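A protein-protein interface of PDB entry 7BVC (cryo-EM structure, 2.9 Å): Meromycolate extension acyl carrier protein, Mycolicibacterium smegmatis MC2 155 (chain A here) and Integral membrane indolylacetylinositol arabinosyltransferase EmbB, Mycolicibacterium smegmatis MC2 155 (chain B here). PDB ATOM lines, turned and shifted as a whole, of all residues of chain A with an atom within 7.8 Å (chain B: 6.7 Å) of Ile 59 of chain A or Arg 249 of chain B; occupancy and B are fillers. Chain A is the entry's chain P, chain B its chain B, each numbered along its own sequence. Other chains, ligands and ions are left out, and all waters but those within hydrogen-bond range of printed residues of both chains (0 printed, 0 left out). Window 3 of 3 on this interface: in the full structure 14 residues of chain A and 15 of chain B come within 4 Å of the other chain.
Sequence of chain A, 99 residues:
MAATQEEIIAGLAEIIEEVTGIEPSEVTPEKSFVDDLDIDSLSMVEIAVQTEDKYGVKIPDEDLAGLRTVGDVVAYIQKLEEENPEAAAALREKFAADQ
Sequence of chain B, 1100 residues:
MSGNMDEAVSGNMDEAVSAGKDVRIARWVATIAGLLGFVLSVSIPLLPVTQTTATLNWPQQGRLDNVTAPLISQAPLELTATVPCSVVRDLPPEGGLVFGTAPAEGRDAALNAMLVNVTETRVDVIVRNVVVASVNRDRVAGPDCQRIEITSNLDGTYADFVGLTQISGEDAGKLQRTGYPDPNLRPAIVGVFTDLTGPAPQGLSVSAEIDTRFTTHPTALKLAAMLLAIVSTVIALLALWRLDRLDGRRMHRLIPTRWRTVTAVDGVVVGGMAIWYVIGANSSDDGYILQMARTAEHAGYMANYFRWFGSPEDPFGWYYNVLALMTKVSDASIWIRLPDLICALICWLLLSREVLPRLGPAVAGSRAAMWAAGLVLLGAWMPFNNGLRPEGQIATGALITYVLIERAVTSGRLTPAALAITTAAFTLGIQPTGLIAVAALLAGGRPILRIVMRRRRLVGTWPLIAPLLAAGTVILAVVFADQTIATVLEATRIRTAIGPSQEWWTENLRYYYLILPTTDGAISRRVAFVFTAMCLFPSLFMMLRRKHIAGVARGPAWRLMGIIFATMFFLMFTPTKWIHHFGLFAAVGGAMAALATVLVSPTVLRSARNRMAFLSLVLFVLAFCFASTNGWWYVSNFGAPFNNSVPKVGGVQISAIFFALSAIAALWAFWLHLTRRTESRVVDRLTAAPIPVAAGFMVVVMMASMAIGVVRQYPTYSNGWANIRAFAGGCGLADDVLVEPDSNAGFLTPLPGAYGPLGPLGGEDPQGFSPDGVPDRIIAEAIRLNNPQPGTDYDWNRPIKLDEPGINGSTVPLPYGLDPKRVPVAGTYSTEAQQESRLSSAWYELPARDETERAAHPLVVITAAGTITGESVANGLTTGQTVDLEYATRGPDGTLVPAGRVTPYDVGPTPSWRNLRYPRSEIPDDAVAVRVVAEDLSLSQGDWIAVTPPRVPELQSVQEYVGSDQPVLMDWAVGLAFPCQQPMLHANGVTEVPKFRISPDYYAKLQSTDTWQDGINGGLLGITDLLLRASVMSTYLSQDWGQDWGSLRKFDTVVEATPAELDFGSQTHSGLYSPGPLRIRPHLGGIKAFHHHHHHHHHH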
ATOM      1  N   MET A  44     -17.532 -12.683  22.894  1.00  0.00           N
ATOM      2  CA  MET A  44     -18.833 -12.270  23.404  1.00  0.00           C
ATOM      3  C   MET A  44     -19.137 -12.932  24.739  1.00  0.00           C
ATOM      4  O   MET A  44     -19.760 -12.314  25.610  1.00  0.00           O
ATOM      5  CB  MET A  44     -19.924 -12.590  22.383  1.00  0.00           C
ATOM      6  CG  MET A  44     -20.056 -11.562  21.274  1.00  0.00           C
ATOM      7  SD  MET A  44     -20.691  -9.985  21.865  1.00  0.00           S
ATOM      8  CE  MET A  44     -22.369 -10.441  22.292  1.00  0.00           C
ATOM      9  N   VAL A  45     -18.691 -14.174  24.927  1.00  0.00           N
ATOM     10  CA  VAL A  45     -18.855 -14.831  26.222  1.00  0.00           C
ATOM     11  C   VAL A  45     -18.068 -14.090  27.297  1.00  0.00           C
ATOM     12  O   VAL A  45     -18.555 -13.881  28.415  1.00  0.00           O
ATOM     13  CB  VAL A  45     -18.435 -16.308  26.134  1.00  0.00           C
ATOM     14  CG1 VAL A  45     -18.570 -16.984  27.489  1.00  0.00           C
ATOM     15  CG2 VAL A  45     -19.265 -17.033  25.093  1.00  0.00           C
ATOM     16  N   GLU A  46     -16.847 -13.667  26.974  1.00  0.00           N
ATOM     17  CA  GLU A  46     -16.044 -12.929  27.943  1.00  0.00           C
ATOM     18  C   GLU A  46     -16.662 -11.569  28.248  1.00  0.00           C
ATOM     19  O   GLU A  46     -16.625 -11.105  29.393  1.00  0.00           O
ATOM     20  CB  GLU A  46     -14.618 -12.769  27.422  1.00  0.00           C
ATOM     21  CG  GLU A  46     -13.656 -12.154  28.418  1.00  0.00           C
ATOM     22  CD  GLU A  46     -12.209 -12.290  27.984  1.00  0.00           C
ATOM     23  OE1 GLU A  46     -11.953 -12.995  26.986  1.00  0.00           O
ATOM     24  OE2 GLU A  46     -11.328 -11.694  28.641  1.00  0.00           O
ATOM     25  N   ILE A  47     -17.232 -10.917  27.233  1.00  0.00           N
ATOM     26  CA  ILE A  47     -17.907  -9.642  27.457  1.00  0.00           C
ATOM     27  C   ILE A  47     -19.119  -9.834  28.359  1.00  0.00           C
ATOM     28  O   ILE A  47     -19.359  -9.042  29.274  1.00  0.00           O
ATOM     29  CB  ILE A  47     -18.293  -8.999  26.112  1.00  0.00           C
ATOM     30  CG1 ILE A  47     -17.041  -8.592  25.334  1.00  0.00           C
ATOM     31  CG2 ILE A  47     -19.191  -7.793  26.332  1.00  0.00           C
ATOM     32  CD1 ILE A  47     -17.326  -8.088  23.943  1.00  0.00           C
ATOM     33  N   ALA A  48     -19.885 -10.904  28.135  1.00  0.00           N
ATOM     34  CA  ALA A  48     -21.052 -11.165  28.970  1.00  0.00           C
ATOM     35  C   ALA A  48     -20.675 -11.603  30.378  1.00  0.00           C
ATOM     36  O   ALA A  48     -21.492 -11.470  31.294  1.00  0.00           O
ATOM     37  CB  ALA A  48     -21.939 -12.226  28.320  1.00  0.00           C
ATOM     38  N   VAL A  49     -19.468 -12.131  30.568  1.00  0.00           N
ATOM     39  CA  VAL A  49     -19.005 -12.455  31.915  1.00  0.00           C
ATOM     40  C   VAL A  49     -18.560 -11.195  32.648  1.00  0.00           C
ATOM     41  O   VAL A  49     -18.959 -10.944  33.792  1.00  0.00           O
ATOM     42  CB  VAL A  49     -17.878 -13.503  31.854  1.00  0.00           C
ATOM     43  CG1 VAL A  49     -17.161 -13.586  33.188  1.00  0.00           C
ATOM     44  CG2 VAL A  49     -18.439 -14.858  31.469  1.00  0.00           C
ATOM     45  N   GLN A  50     -17.732 -10.377  31.995  1.00  0.00           N
ATOM     46  CA  GLN A  50     -17.273  -9.139  32.616  1.00  0.00           C
ATOM     47  C   GLN A  50     -18.397  -8.126  32.792  1.00  0.00           C
ATOM     48  O   GLN A  50     -18.263  -7.210  33.608  1.00  0.00           O
ATOM     49  CB  GLN A  50     -16.140  -8.525  31.796  1.00  0.00           C
ATOM     50  CG  GLN A  50     -14.879  -9.365  31.773  1.00  0.00           C
ATOM     51  CD  GLN A  50     -13.659  -8.566  31.372  1.00  0.00           C
ATOM     52  OE1 GLN A  50     -13.696  -7.336  31.332  1.00  0.00           O
ATOM     53  NE2 GLN A  50     -12.568  -9.259  31.071  1.00  0.00           N
ATOM     54  N   THR A  51     -19.492  -8.262  32.045  1.00  0.00           N
ATOM     55  CA  THR A  51     -20.658  -7.423  32.290  1.00  0.00           C
ATOM     56  C   THR A  51     -21.279  -7.746  33.641  1.00  0.00           C
ATOM     57  O   THR A  51     -21.572  -6.846  34.434  1.00  0.00           O
ATOM     58  CB  THR A  51     -21.684  -7.607  31.172  1.00  0.00           C
ATOM     59  OG1 THR A  51     -21.176  -7.049  29.956  1.00  0.00           O
ATOM     60  CG2 THR A  51     -22.989  -6.919  31.532  1.00  0.00           C
ATOM     61  N   GLU A  52     -21.476  -9.035  33.924  1.00  0.00           N
ATOM     62  CA  GLU A  52     -22.048  -9.429  35.205  1.00  0.00           C
ATOM     63  C   GLU A  52     -21.074  -9.186  36.349  1.00  0.00           C
ATOM     64  O   GLU A  52     -21.501  -8.910  37.475  1.00  0.00           O
ATOM     65  CB  GLU A  52     -22.468 -10.897  35.169  1.00  0.00           C
ATOM     66  CG  GLU A  52     -23.146 -11.367  36.445  1.00  0.00           C
ATOM     67  CD  GLU A  52     -23.465 -12.846  36.435  1.00  0.00           C
ATOM     68  OE1 GLU A  52     -22.725 -13.612  35.781  1.00  0.00           O
ATOM     69  OE2 GLU A  52     -24.456 -13.241  37.082  1.00  0.00           O
ATOM     70  N   ASP A  53     -19.773  -9.268  36.085  1.00  0.00           N
ATOM     71  CA  ASP A  53     -18.791  -9.040  37.137  1.00  0.00           C
ATOM     72  C   ASP A  53     -18.630  -7.569  37.503  1.00  0.00           C
ATOM     73  O   ASP A  53     -17.848  -7.259  38.408  1.00  0.00           O
ATOM     74  CB  ASP A  53     -17.439  -9.626  36.726  1.00  0.00           C
ATOM     75  CG  ASP A  53     -17.455 -11.143  36.678  1.00  0.00           C
ATOM     76  OD1 ASP A  53     -18.473 -11.739  37.090  1.00  0.00           O
ATOM     77  OD2 ASP A  53     -16.454 -11.740  36.232  1.00  0.00           O
ATOM     78  N   GLY A  56     -24.510  -6.449  38.160  1.00  0.00           N
ATOM     79  CA  GLY A  56     -25.145  -7.752  38.197  1.00  0.00           C
ATOM     80  C   GLY A  56     -26.202  -7.877  37.121  1.00  0.00           C
ATOM     81  O   GLY A  56     -27.322  -7.381  37.266  1.00  0.00           O
ATOM     82  N   VAL A  57     -25.846  -8.570  36.039  1.00  0.00           N
ATOM     83  CA  VAL A  57     -26.711  -8.787  34.884  1.00  0.00           C
ATOM     84  C   VAL A  57     -26.346 -10.137  34.285  1.00  0.00           C
ATOM     85  O   VAL A  57     -25.244 -10.309  33.753  1.00  0.00           O
ATOM     86  CB  VAL A  57     -26.572  -7.672  33.827  1.00  0.00           C
ATOM     87  CG1 VAL A  57     -27.338  -8.044  32.571  1.00  0.00           C
ATOM     88  CG2 VAL A  57     -27.070  -6.334  34.353  1.00  0.00           C
ATOM     89  N   LYS A  58     -27.259 -11.097  34.353  1.00  0.00           N
ATOM     90  CA  LYS A  58     -27.015 -12.432  33.813  1.00  0.00           C
ATOM     91  C   LYS A  58     -27.680 -12.519  32.445  1.00  0.00           C
ATOM     92  O   LYS A  58     -28.897 -12.692  32.341  1.00  0.00           O
ATOM     93  CB  LYS A  58     -27.528 -13.510  34.762  1.00  0.00           C
ATOM     94  CG  LYS A  58     -27.087 -14.914  34.386  1.00  0.00           C
ATOM     95  CD  LYS A  58     -27.086 -15.843  35.586  1.00  0.00           C
ATOM     96  CE  LYS A  58     -25.672 -16.072  36.098  1.00  0.00           C
ATOM     97  NZ  LYS A  58     -25.654 -16.625  37.479  1.00  0.00           N
ATOM     98  N   ILE A  59     -26.874 -12.388  31.395  1.00  0.00           N
ATOM     99  CA  ILE A  59     -27.341 -12.537  30.021  1.00  0.00           C
ATOM    100  C   ILE A  59     -27.199 -14.009  29.644  1.00  0.00           C
ATOM    101  O   ILE A  59     -26.069 -14.465  29.401  1.00  0.00           O
ATOM    102  CB  ILE A  59     -26.554 -11.641  29.057  1.00  0.00           C
ATOM    103  CG1 ILE A  59     -26.547 -10.197  29.558  1.00  0.00           C
ATOM    104  CG2 ILE A  59     -27.143 -11.717  27.659  1.00  0.00           C
ATOM    105  CD1 ILE A  59     -25.738  -9.262  28.696  1.00  0.00           C
ATOM    106  N   PRO A  60     -28.285 -14.775  29.588  1.00  0.00           N
ATOM    107  CA  PRO A  60     -28.159 -16.205  29.299  1.00  0.00           C
ATOM    108  C   PRO A  60     -27.816 -16.448  27.840  1.00  0.00           C
ATOM    109  O   PRO A  60     -28.182 -15.673  26.953  1.00  0.00           O
ATOM    110  CB  PRO A  60     -29.545 -16.756  29.644  1.00  0.00           C
ATOM    111  CG  PRO A  60     -30.462 -15.609  29.381  1.00  0.00           C
ATOM    112  CD  PRO A  60     -29.692 -14.358  29.725  1.00  0.00           C
ATOM    113  N   ASP A  61     -27.100 -17.549  27.598  1.00  0.00           N
ATOM    114  CA  ASP A  61     -26.760 -17.937  26.234  1.00  0.00           C
ATOM    115  C   ASP A  61     -27.989 -18.208  25.377  1.00  0.00           C
ATOM    116  O   ASP A  61     -27.856 -18.333  24.155  1.00  0.00           O
ATOM    117  CB  ASP A  61     -25.847 -19.165  26.253  1.00  0.00           C
ATOM    118  CG  ASP A  61     -26.396 -20.287  27.111  1.00  0.00           C
ATOM    119  OD1 ASP A  61     -27.354 -20.043  27.872  1.00  0.00           O
ATOM    120  OD2 ASP A  61     -25.866 -21.415  27.025  1.00  0.00           O
ATOM    121  N   GLU A  62     -29.174 -18.306  25.985  1.00  0.00           N
ATOM    122  CA  GLU A  62     -30.406 -18.337  25.204  1.00  0.00           C
ATOM    123  C   GLU A  62     -30.586 -17.048  24.415  1.00  0.00           C
ATOM    124  O   GLU A  62     -31.114 -17.063  23.296  1.00  0.00           O
ATOM    125  CB  GLU A  62     -31.599 -18.572  26.131  1.00  0.00           C
ATOM    126  CG  GLU A  62     -32.951 -18.613  25.434  1.00  0.00           C
ATOM    127  CD  GLU A  62     -33.093 -19.795  24.498  1.00  0.00           C
ATOM    128  OE1 GLU A  62     -32.418 -20.823  24.724  1.00  0.00           O
ATOM    129  OE2 GLU A  62     -33.883 -19.699  23.534  1.00  0.00           O
ATOM    130  N   ASP A  63     -30.146 -15.921  24.977  1.00  0.00           N
ATOM    131  CA  ASP A  63     -30.287 -14.624  24.338  1.00  0.00           C
ATOM    132  C   ASP A  63     -28.975 -14.055  23.816  1.00  0.00           C
ATOM    133  O   ASP A  63     -29.003 -13.092  23.044  1.00  0.00           O
ATOM    134  CB  ASP A  63     -30.916 -13.619  25.315  1.00  0.00           C
ATOM    135  CG  ASP A  63     -31.663 -12.506  24.608  1.00  0.00           C
ATOM    136  OD1 ASP A  63     -31.689 -12.501  23.360  1.00  0.00           O
ATOM    137  OD2 ASP A  63     -32.228 -11.634  25.300  1.00  0.00           O
ATOM    138  N   LEU A  64     -27.831 -14.617  24.213  1.00  0.00           N
ATOM    139  CA  LEU A  64     -26.542 -14.110  23.756  1.00  0.00           C
ATOM    140  C   LEU A  64     -26.310 -14.334  22.267  1.00  0.00           C
ATOM    141  O   LEU A  64     -25.384 -13.738  21.708  1.00  0.00           O
ATOM    142  CB  LEU A  64     -25.411 -14.760  24.555  1.00  0.00           C
ATOM    143  CG  LEU A  64     -24.111 -13.961  24.682  1.00  0.00           C
ATOM    144  CD1 LEU A  64     -24.401 -12.523  25.083  1.00  0.00           C
ATOM    145  CD2 LEU A  64     -23.172 -14.622  25.676  1.00  0.00           C
ATOM    146  N   ALA A  65     -27.119 -15.167  21.617  1.00  0.00           N
ATOM    147  CA  ALA A  65     -26.975 -15.398  20.187  1.00  0.00           C
ATOM    148  C   ALA A  65     -27.783 -14.418  19.349  1.00  0.00           C
ATOM    149  O   ALA A  65     -27.421 -14.156  18.197  1.00  0.00           O
ATOM    150  CB  ALA A  65     -27.391 -16.831  19.839  1.00  0.00           C
ATOM    151  N   LEU A  67     -28.030 -11.229  19.611  1.00  0.00           N
ATOM    152  CA  LEU A  67     -27.479  -9.876  19.612  1.00  0.00           C
ATOM    153  C   LEU A  67     -26.509  -9.762  18.442  1.00  0.00           C
ATOM    154  O   LEU A  67     -25.364 -10.214  18.524  1.00  0.00           O
ATOM    155  CB  LEU A  67     -26.796  -9.568  20.940  1.00  0.00           C
ATOM    156  CG  LEU A  67     -27.607  -9.835  22.209  1.00  0.00           C
ATOM    157  CD1 LEU A  67     -26.887  -9.285  23.426  1.00  0.00           C
ATOM    158  CD2 LEU A  67     -29.000  -9.240  22.098  1.00  0.00           C
ATOM    159  N   VAL A  73     -28.203  -4.643  21.572  1.00  0.00           N
ATOM    160  CA  VAL A  73     -27.782  -4.649  22.970  1.00  0.00           C
ATOM    161  C   VAL A  73     -28.482  -3.541  23.746  1.00  0.00           C
ATOM    162  O   VAL A  73     -28.978  -3.760  24.862  1.00  0.00           O
ATOM    163  CB  VAL A  73     -26.251  -4.521  23.067  1.00  0.00           C
ATOM    164  CG1 VAL A  73     -25.837  -4.155  24.479  1.00  0.00           C
ATOM    165  CG2 VAL A  73     -25.585  -5.813  22.636  1.00  0.00           C
ATOM    166  N   TYR A  76     -32.137  -4.491  24.229  1.00  0.00           N
ATOM    167  CA  TYR A  76     -32.296  -5.545  25.226  1.00  0.00           C
ATOM    168  C   TYR A  76     -32.149  -4.991  26.637  1.00  0.00           C
ATOM    169  O   TYR A  76     -32.976  -5.266  27.518  1.00  0.00           O
ATOM    170  CB  TYR A  76     -31.274  -6.651  24.961  1.00  0.00           C
ATOM    171  CG  TYR A  76     -31.110  -7.659  26.074  1.00  0.00           C
ATOM    172  CD1 TYR A  76     -32.169  -8.459  26.480  1.00  0.00           C
ATOM    173  CD2 TYR A  76     -29.884  -7.828  26.704  1.00  0.00           C
ATOM    174  CE1 TYR A  76     -32.016  -9.387  27.493  1.00  0.00           C
ATOM    175  CE2 TYR A  76     -29.721  -8.755  27.717  1.00  0.00           C
ATOM    176  CZ  TYR A  76     -30.791  -9.530  28.107  1.00  0.00           C
ATOM    177  OH  TYR A  76     -30.637 -10.454  29.115  1.00  0.00           O
ATOM    178  N   ILE A  77     -31.104  -4.195  26.870  1.00  0.00           N
ATOM    179  CA  ILE A  77     -30.908  -3.617  28.196  1.00  0.00           C
ATOM    180  C   ILE A  77     -32.063  -2.689  28.549  1.00  0.00           C
ATOM    181  O   ILE A  77     -32.585  -2.729  29.672  1.00  0.00           O
ATOM    182  CB  ILE A  77     -29.550  -2.898  28.275  1.00  0.00           C
ATOM    183  CG1 ILE A  77     -28.431  -3.908  28.527  1.00  0.00           C
ATOM    184  CG2 ILE A  77     -29.561  -1.853  29.376  1.00  0.00           C
ATOM    185  CD1 ILE A  77     -27.066  -3.280  28.682  1.00  0.00           C
ATOM    186  N   LEU A  80     -35.229  -4.778  29.402  1.00  0.00           N
ATOM    187  CA  LEU A  80     -35.164  -5.491  30.671  1.00  0.00           C
ATOM    188  C   LEU A  80     -35.142  -4.541  31.861  1.00  0.00           C
ATOM    189  O   LEU A  80     -35.615  -4.914  32.939  1.00  0.00           O
ATOM    190  CB  LEU A  80     -33.947  -6.422  30.715  1.00  0.00           C
ATOM    191  CG  LEU A  80     -32.525  -5.863  30.765  1.00  0.00           C
ATOM    192  CD1 LEU A  80     -32.062  -5.626  32.200  1.00  0.00           C
ATOM    193  CD2 LEU A  80     -31.569  -6.794  30.047  1.00  0.00           C
ATOM    194  N   ASP B 244     -18.822 -25.716  38.882  1.00  0.00           N
ATOM    195  CA  ASP B 244     -18.613 -24.626  37.936  1.00  0.00           C
ATOM    196  C   ASP B 244     -19.803 -24.446  37.006  1.00  0.00           C
ATOM    197  O   ASP B 244     -20.047 -23.338  36.520  1.00  0.00           O
ATOM    198  CB  ASP B 244     -17.350 -24.875  37.115  1.00  0.00           C
ATOM    199  CG  ASP B 244     -16.088 -24.486  37.852  1.00  0.00           C
ATOM    200  OD1 ASP B 244     -16.193 -23.971  38.984  1.00  0.00           O
ATOM    201  OD2 ASP B 244     -14.989 -24.697  37.297  1.00  0.00           O
ATOM    202  N   ARG B 245     -20.557 -25.514  36.756  1.00  0.00           N
ATOM    203  CA  ARG B 245     -21.664 -25.448  35.808  1.00  0.00           C
ATOM    204  C   ARG B 245     -22.878 -24.729  36.385  1.00  0.00           C
ATOM    205  O   ARG B 245     -23.975 -24.816  35.827  1.00  0.00           O
ATOM    206  CB  ARG B 245     -22.067 -26.851  35.354  1.00  0.00           C
ATOM    207  CG  ARG B 245     -21.336 -27.336  34.119  1.00  0.00           C
ATOM    208  CD  ARG B 245     -21.497 -28.832  33.940  1.00  0.00           C
ATOM    209  NE  ARG B 245     -22.819 -29.185  33.434  1.00  0.00           N
ATOM    210  CZ  ARG B 245     -23.099 -29.374  32.149  1.00  0.00           C
ATOM    211  NH1 ARG B 245     -22.147 -29.244  31.234  1.00  0.00           N
ATOM    212  NH2 ARG B 245     -24.329 -29.693  31.777  1.00  0.00           N
ATOM    213  N   LEU B 246     -22.699 -24.025  37.506  1.00  0.00           N
ATOM    214  CA  LEU B 246     -23.816 -23.314  38.118  1.00  0.00           C
ATOM    215  C   LEU B 246     -24.217 -22.080  37.318  1.00  0.00           C
ATOM    216  O   LEU B 246     -25.373 -21.648  37.395  1.00  0.00           O
ATOM    217  CB  LEU B 246     -23.469 -22.917  39.550  1.00  0.00           C
ATOM    218  CG  LEU B 246     -23.637 -23.996  40.620  1.00  0.00           C
ATOM    219  CD1 LEU B 246     -23.193 -23.473  41.972  1.00  0.00           C
ATOM    220  CD2 LEU B 246     -25.078 -24.467  40.671  1.00  0.00           C
ATOM    221  N   ASP B 247     -23.292 -21.499  36.555  1.00  0.00           N
ATOM    222  CA  ASP B 247     -23.599 -20.281  35.814  1.00  0.00           C
ATOM    223  C   ASP B 247     -24.551 -20.513  34.647  1.00  0.00           C
ATOM    224  O   ASP B 247     -24.945 -19.540  33.997  1.00  0.00           O
ATOM    225  CB  ASP B 247     -22.309 -19.630  35.313  1.00  0.00           C
ATOM    226  CG  ASP B 247     -21.355 -20.627  34.691  1.00  0.00           C
ATOM    227  OD1 ASP B 247     -21.721 -21.813  34.582  1.00  0.00           O
ATOM    228  OD2 ASP B 247     -20.235 -20.224  34.316  1.00  0.00           O
ATOM    229  N   GLY B 248     -24.926 -21.758  34.366  1.00  0.00           N
ATOM    230  CA  GLY B 248     -25.925 -22.023  33.350  1.00  0.00           C
ATOM    231  C   GLY B 248     -25.458 -21.860  31.923  1.00  0.00           C
ATOM    232  O   GLY B 248     -26.266 -21.526  31.051  1.00  0.00           O
ATOM    233  N   ARG B 249     -24.177 -22.085  31.655  1.00  0.00           N
ATOM    234  CA  ARG B 249     -23.631 -22.007  30.308  1.00  0.00           C
ATOM    235  C   ARG B 249     -23.143 -23.384  29.883  1.00  0.00           C
ATOM    236  O   ARG B 249     -22.391 -24.034  30.616  1.00  0.00           O
ATOM    237  CB  ARG B 249     -22.492 -20.989  30.233  1.00  0.00           C
ATOM    238  CG  ARG B 249     -22.936 -19.565  30.512  1.00  0.00           C
ATOM    239  CD  ARG B 249     -21.838 -18.561  30.216  1.00  0.00           C
ATOM    240  NE  ARG B 249     -22.364 -17.200  30.162  1.00  0.00           N
ATOM    241  CZ  ARG B 249     -22.311 -16.336  31.172  1.00  0.00           C
ATOM    242  NH1 ARG B 249     -21.751 -16.686  32.321  1.00  0.00           N
ATOM    243  NH2 ARG B 249     -22.820 -15.121  31.031  1.00  0.00           N
ATOM    244  N   ARG B 250     -23.581 -23.826  28.708  1.00  0.00           N
ATOM    245  CA  ARG B 250     -23.209 -25.117  28.157  1.00  0.00           C
ATOM    246  C   ARG B 250     -22.557 -24.923  26.796  1.00  0.00           C
ATOM    247  O   ARG B 250     -22.699 -23.877  26.159  1.00  0.00           O
ATOM    248  CB  ARG B 250     -24.427 -26.040  28.014  1.00  0.00           C
ATOM    249  CG  ARG B 250     -25.464 -25.903  29.115  1.00  0.00           C
ATOM    250  CD  ARG B 250     -24.902 -26.306  30.466  1.00  0.00           C
ATOM    251  NE  ARG B 250     -25.960 -26.590  31.429  1.00  0.00           N
ATOM    252  CZ  ARG B 250     -25.793 -26.573  32.747  1.00  0.00           C
ATOM    253  NH1 ARG B 250     -24.606 -26.280  33.261  1.00  0.00           N
ATOM    254  NH2 ARG B 250     -26.812 -26.844  33.549  1.00  0.00           N
ATOM    255  N   MET B 251     -21.835 -25.947  26.352  1.00  0.00           N
ATOM    256  CA  MET B 251     -21.261 -25.929  25.016  1.00  0.00           C
ATOM    257  C   MET B 251     -22.355 -26.155  23.981  1.00  0.00           C
ATOM    258  O   MET B 251     -23.236 -27.000  24.157  1.00  0.00           O
ATOM    259  CB  MET B 251     -20.162 -26.988  24.881  1.00  0.00           C
ATOM    260  CG  MET B 251     -20.654 -28.427  24.820  1.00  0.00           C
ATOM    261  SD  MET B 251     -19.320 -29.639  24.852  1.00  0.00           S
ATOM    262  CE  MET B 251     -18.608 -29.406  23.228  1.00  0.00           C
ATOM    263  N   SER B 411     -13.773 -17.936  30.041  1.00  0.00           N
ATOM    264  CA  SER B 411     -15.075 -18.437  30.466  1.00  0.00           C
ATOM    265  C   SER B 411     -15.385 -18.129  31.923  1.00  0.00           C
ATOM    266  O   SER B 411     -16.553 -18.193  32.320  1.00  0.00           O
ATOM    267  CB  SER B 411     -15.157 -19.945  30.233  1.00  0.00           C
ATOM    268  OG  SER B 411     -14.236 -20.637  31.058  1.00  0.00           O
ATOM    269  N   ARG B 413     -14.141 -19.837  34.738  1.00  0.00           N
ATOM    270  CA  ARG B 413     -14.334 -21.090  35.451  1.00  0.00           C
ATOM    271  C   ARG B 413     -13.000 -21.562  36.013  1.00  0.00           C
ATOM    272  O   ARG B 413     -11.939 -21.011  35.711  1.00  0.00           O
ATOM    273  CB  ARG B 413     -14.939 -22.165  34.541  1.00  0.00           C
ATOM    274  CG  ARG B 413     -16.383 -21.909  34.159  1.00  0.00           C
ATOM    275  CD  ARG B 413     -16.948 -23.055  33.339  1.00  0.00           C
ATOM    276  NE  ARG B 413     -18.388 -22.923  33.139  1.00  0.00           N
ATOM    277  CZ  ARG B 413     -19.132 -23.802  32.479  1.00  0.00           C
ATOM    278  NH1 ARG B 413     -18.575 -24.883  31.954  1.00  0.00           N
ATOM    279  NH2 ARG B 413     -20.435 -23.603  32.344  1.00  0.00           N
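NH1 of Arg 250 of chain B sits at hydrogen-bond distance from O of Arg 245 of chain B (3.0 Å).
The guanidinium group (NH2) of Arg 413 of chain B sits at hydrogen-bond distance from the backbone carbonyl oxygen (O) of Arg 249 of chain B.
Ala 48 of chain A touches Arg 249 of chain B.
NH1 of Arg 249 of chain B touches CG2 of Val 49 of chain A, at 3.9 Å.
Ser 411 of chain B touches Val 49 of chain A.
Ile 59 of chain A touches Arg 249 of chain B.
OD1 of Asp 61 of chain A touches O of Gly 248 of chain B (3.7 Å).
OD2 of Asp 61 of chain A touches N of Arg 250 of chain B, at 3.7 Å.
Of chain B, only Arg 249 comes within 4 Å of Ile 59 of chain A.
Of the printed residues of chain A, Arg 249 of chain B touches Ala 48 (3.9 Å), Val 49 (3.9 Å) and Ile 59 (3.7 Å).
Of chain A, only Asp 61 comes within 4 Å of Gly 248 of chain B.
Of the printed residues of chain B, Val 49 of chain A touches Arg 249 and Ser 411.
Of the printed residues of chain B, Asp 61 of chain A touches Gly 248 (3.7 Å) and Arg 250 (3.7 Å).
Of the printed residues of chain B, Ala 48 of chain A touches Arg 249 (3.9 Å).
Of the printed residues of chain A, Ser 411 of chain B touches Val 49.
Of the printed residues of chain A, Arg 250 of chain B touches Asp 61.
The nearest printed residue of chain B that does not touch Ile 59 of chain A is Asp 247 of chain B (6.9 Å).
The nearest printed residue of chain A that does not touch Ser 411 of chain B is Val 45 of chain A (4.8 Å).
Printed residues of chain A that touch a printed residue of chain B: Ala 48, Val 49, Ile 59 and Asp 61.
Among the printed residues, 6 pairs touch across the chains.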
